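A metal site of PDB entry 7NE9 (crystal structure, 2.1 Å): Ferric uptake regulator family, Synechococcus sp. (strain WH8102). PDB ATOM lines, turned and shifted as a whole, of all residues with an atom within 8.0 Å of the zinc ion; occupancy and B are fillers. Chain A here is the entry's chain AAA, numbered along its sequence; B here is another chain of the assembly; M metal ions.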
ATOM      1  N   THR A  82      -5.109 -10.079  -7.533  1.00  0.00           N
ATOM      2  CA  THR A  82      -5.349  -8.986  -6.564  1.00  0.00           C
ATOM      3  C   THR A  82      -5.853  -7.786  -7.349  1.00  0.00           C
ATOM      4  O   THR A  82      -5.211  -7.421  -8.367  1.00  0.00           O
ATOM      5  CB  THR A  82      -4.083  -8.691  -5.753  1.00  0.00           C
ATOM      6  OG1 THR A  82      -3.693  -9.899  -5.096  1.00  0.00           O
ATOM      7  CG2 THR A  82      -4.293  -7.569  -4.744  1.00  0.00           C
ATOM      8  N   CYS A  83      -6.953  -7.208  -6.899  1.00  0.00           N
ATOM      9  CA  CYS A  83      -7.469  -5.922  -7.431  1.00  0.00           C
ATOM     10  C   CYS A  83      -6.575  -4.774  -6.927  1.00  0.00           C
ATOM     11  O   CYS A  83      -6.400  -4.638  -5.726  1.00  0.00           O
ATOM     12  CB  CYS A  83      -8.913  -5.706  -7.019  1.00  0.00           C
ATOM     13  SG  CYS A  83      -9.603  -4.194  -7.730  1.00  0.00           S
ATOM     14  N   VAL A  84      -6.062  -3.963  -7.841  1.00  0.00           N
ATOM     15  CA  VAL A  84      -5.134  -2.839  -7.522  1.00  0.00           C
ATOM     16  C   VAL A  84      -5.963  -1.688  -6.905  1.00  0.00           C
ATOM     17  O   VAL A  84      -5.363  -0.794  -6.318  1.00  0.00           O
ATOM     18  CB  VAL A  84      -4.372  -2.366  -8.768  1.00  0.00           C
ATOM     19  CG1 VAL A  84      -3.508  -3.489  -9.321  1.00  0.00           C
ATOM     20  CG2 VAL A  84      -5.291  -1.799  -9.842  1.00  0.00           C
ATOM     21  N   ASP A  85      -7.273  -1.692  -7.104  1.00  0.00           N
ATOM     22  CA  ASP A  85      -8.178  -0.615  -6.630  1.00  0.00           C
ATOM     23  C   ASP A  85      -8.574  -0.914  -5.181  1.00  0.00           C
ATOM     24  O   ASP A  85      -8.089  -0.199  -4.286  1.00  0.00           O
ATOM     25  CB  ASP A  85      -9.377  -0.440  -7.562  1.00  0.00           C
ATOM     26  CG  ASP A  85     -10.127   0.853  -7.314  1.00  0.00           C
ATOM     27  OD1 ASP A  85      -9.838   1.516  -6.318  1.00  0.00           O
ATOM     28  OD2 ASP A  85     -10.983   1.197  -8.125  1.00  0.00           O
ATOM     29  N   CYS A  86      -9.370  -1.970  -4.940  1.00  0.00           N
ATOM     30  CA  CYS A  86      -9.951  -2.296  -3.617  1.00  0.00           C
ATOM     31  C   CYS A  86      -9.061  -3.269  -2.820  1.00  0.00           C
ATOM     32  O   CYS A  86      -9.361  -3.462  -1.627  1.00  0.00           O
ATOM     33  CB  CYS A  86     -11.355  -2.833  -3.786  1.00  0.00           C
ATOM     34  SG  CYS A  86     -11.425  -4.514  -4.491  1.00  0.00           S
ATOM     35  N   GLY A  87      -8.026  -3.881  -3.419  1.00  0.00           N
ATOM     36  CA  GLY A  87      -7.125  -4.795  -2.683  1.00  0.00           C
ATOM     37  C   GLY A  87      -7.723  -6.185  -2.467  1.00  0.00           C
ATOM     38  O   GLY A  87      -7.039  -7.020  -1.871  1.00  0.00           O
ATOM     39  N   THR A  88      -8.921  -6.485  -2.950  1.00  0.00           N
ATOM     40  CA  THR A  88      -9.498  -7.855  -2.830  1.00  0.00           C
ATOM     41  C   THR A  88      -8.578  -8.844  -3.561  1.00  0.00           C
ATOM     42  O   THR A  88      -8.032  -8.487  -4.610  1.00  0.00           O
ATOM     43  CB  THR A  88     -10.956  -7.896  -3.313  1.00  0.00           C
ATOM     44  OG1 THR A  88     -11.451  -9.140  -2.822  1.00  0.00           O
ATOM     45  CG2 THR A  88     -11.131  -7.863  -4.813  1.00  0.00           C
ATOM     46  N   THR A  89      -8.401 -10.045  -3.008  1.00  0.00           N
ATOM     47  CA  THR A  89      -7.451 -11.069  -3.508  1.00  0.00           C
ATOM     48  C   THR A  89      -8.137 -12.426  -3.583  1.00  0.00           C
ATOM     49  O   THR A  89      -8.953 -12.710  -2.718  1.00  0.00           O
ATOM     50  CB  THR A  89      -6.171 -11.074  -2.649  1.00  0.00           C
ATOM     51  OG1 THR A  89      -5.157 -11.802  -3.357  1.00  0.00           O
ATOM     52  CG2 THR A  89      -6.334 -11.718  -1.291  1.00  0.00           C
ATOM     53  N   GLY A 121      -4.961  -6.626 -11.318  1.00  0.00           N
ATOM     54  CA  GLY A 121      -5.932  -6.058 -12.257  1.00  0.00           C
ATOM     55  C   GLY A 121      -7.064  -5.395 -11.514  1.00  0.00           C
ATOM     56  O   GLY A 121      -6.862  -4.952 -10.364  1.00  0.00           O
ATOM     57  N   PHE A 122      -8.224  -5.297 -12.159  1.00  0.00           N
ATOM     58  CA  PHE A 122      -9.462  -4.758 -11.553  1.00  0.00           C
ATOM     59  C   PHE A 122     -10.458  -5.900 -11.402  1.00  0.00           C
ATOM     60  O   PHE A 122     -10.678  -6.623 -12.374  1.00  0.00           O
ATOM     61  CB  PHE A 122     -10.051  -3.665 -12.434  1.00  0.00           C
ATOM     62  CG  PHE A 122      -9.191  -2.450 -12.634  1.00  0.00           C
ATOM     63  CD1 PHE A 122      -8.824  -1.644 -11.561  1.00  0.00           C
ATOM     64  CD2 PHE A 122      -8.787  -2.071 -13.914  1.00  0.00           C
ATOM     65  CE1 PHE A 122      -8.041  -0.513 -11.763  1.00  0.00           C
ATOM     66  CE2 PHE A 122      -8.025  -0.928 -14.115  1.00  0.00           C
ATOM     67  CZ  PHE A 122      -7.646  -0.166 -13.041  1.00  0.00           C
ATOM     68  N   CYS A 123     -11.030  -6.031 -10.206  1.00  0.00           N
ATOM     69  CA  CYS A 123     -12.165  -6.958  -9.944  1.00  0.00           C
ATOM     70  C   CYS A 123     -13.433  -6.403 -10.622  1.00  0.00           C
ATOM     71  O   CYS A 123     -13.415  -5.265 -11.117  1.00  0.00           O
ATOM     72  CB  CYS A 123     -12.342  -7.147  -8.446  1.00  0.00           C
ATOM     73  SG  CYS A 123     -13.146  -5.742  -7.638  1.00  0.00           S
ATOM     74  N   SER A 124     -14.511  -7.208 -10.634  1.00  0.00           N
ATOM     75  CA  SER A 124     -15.844  -6.904 -11.241  1.00  0.00           C
ATOM     76  C   SER A 124     -16.343  -5.528 -10.808  1.00  0.00           C
ATOM     77  O   SER A 124     -16.736  -4.738 -11.672  1.00  0.00           O
ATOM     78  CB  SER A 124     -16.864  -7.964 -10.872  1.00  0.00           C
ATOM     79  OG  SER A 124     -16.479  -9.252 -11.321  1.00  0.00           O
ATOM     80  N   SER A 125     -16.335  -5.272  -9.491  1.00  0.00           N
ATOM     81  CA  SER A 125     -16.820  -4.009  -8.874  1.00  0.00           C
ATOM     82  C   SER A 125     -16.023  -2.798  -9.373  1.00  0.00           C
ATOM     83  O   SER A 125     -16.622  -1.726  -9.503  1.00  0.00           O
ATOM     84  CB  SER A 125     -16.766  -4.079  -7.375  1.00  0.00           C
ATOM     85  OG  SER A 125     -17.253  -5.318  -6.918  1.00  0.00           O
ATOM     86  N   CYS A 126     -14.715  -2.938  -9.618  1.00  0.00           N
ATOM     87  CA  CYS A 126     -13.783  -1.786  -9.803  1.00  0.00           C
ATOM     88  C   CYS A 126     -13.542  -1.485 -11.293  1.00  0.00           C
ATOM     89  O   CYS A 126     -13.059  -0.383 -11.569  1.00  0.00           O
ATOM     90  CB  CYS A 126     -12.441  -2.049  -9.111  1.00  0.00           C
ATOM     91  SG  CYS A 126     -12.545  -2.073  -7.298  1.00  0.00           S
ATOM     92  N   ARG A 127     -13.834  -2.405 -12.221  1.00  0.00           N
ATOM     93  CA  ARG A 127     -13.344  -2.334 -13.626  1.00  0.00           C
ATOM     94  C   ARG A 127     -14.036  -1.199 -14.382  1.00  0.00           C
ATOM     95  O   ARG A 127     -15.257  -1.177 -14.446  1.00  0.00           O
ATOM     96  CB  ARG A 127     -13.556  -3.659 -14.371  1.00  0.00           C
ATOM     97  CG  ARG A 127     -14.922  -4.275 -14.114  1.00  0.00           C
ATOM     98  CD  ARG A 127     -15.415  -5.199 -15.196  1.00  0.00           C
ATOM     99  NE  ARG A 127     -14.873  -6.539 -14.984  1.00  0.00           N
ATOM    100  CZ  ARG A 127     -14.141  -7.249 -15.853  1.00  0.00           C
ATOM    101  NH1 ARG A 127     -13.845  -6.756 -17.046  1.00  0.00           N
ATOM    102  NH2 ARG A 127     -13.729  -8.453 -15.513  1.00  0.00           N
ATOM    103  N   PHE B 110     -12.433 -11.070 -13.946  1.00  0.00           N
ATOM    104  CA  PHE B 110     -11.398 -10.175 -13.373  1.00  0.00           C
ATOM    105  C   PHE B 110     -10.637  -9.573 -14.556  1.00  0.00           C
ATOM    106  O   PHE B 110     -10.266 -10.360 -15.446  1.00  0.00           O
ATOM    107  CB  PHE B 110     -10.498 -11.060 -12.503  1.00  0.00           C
ATOM    108  CG  PHE B 110      -9.436 -10.326 -11.752  1.00  0.00           C
ATOM    109  CD1 PHE B 110      -9.705  -9.793 -10.494  1.00  0.00           C
ATOM    110  CD2 PHE B 110      -8.166 -10.170 -12.289  1.00  0.00           C
ATOM    111  CE1 PHE B 110      -8.733  -9.118  -9.785  1.00  0.00           C
ATOM    112  CE2 PHE B 110      -7.184  -9.494 -11.577  1.00  0.00           C
ATOM    113  CZ  PHE B 110      -7.471  -8.975 -10.328  1.00  0.00           C
HETATM  114 ZN    ZN M   1     -11.717  -4.185  -6.738  1.00  0.00          ZN
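SG of Cys 86 binds the zinc ion, at 2.3 Å.
The zinc ion is bound by SG of Cys 123, 2.3 Å away.
The zinc ion is bound by SG of Cys 83 (2.3 Å).
The zinc ion is bound by SG of Cys 126, at 2.3 Å.
The side-chain sulfur (SG) of Cys 86 lies close to the backbone NH (N) of Thr 88, 3.5 Å away.
The side-chain sulfur (SG) of Cys 123 sits close to the backbone NH (N) of Ser 125 (3.7 Å).
The backbone NH (N) of Cys 83 lies within hydrogen-bond range of the backbone carbonyl oxygen (O) of Thr 88 (2.8 Å).
The backbone NH (N) of Asp 85 lies close to the side-chain sulfur (SG) of Cys 83, 3.5 Å away.
SG of Cys 126 lies close to OD2 of Asp 85.
Of the 16 residues printed, 4 come within 4 Å of the zinc ion.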
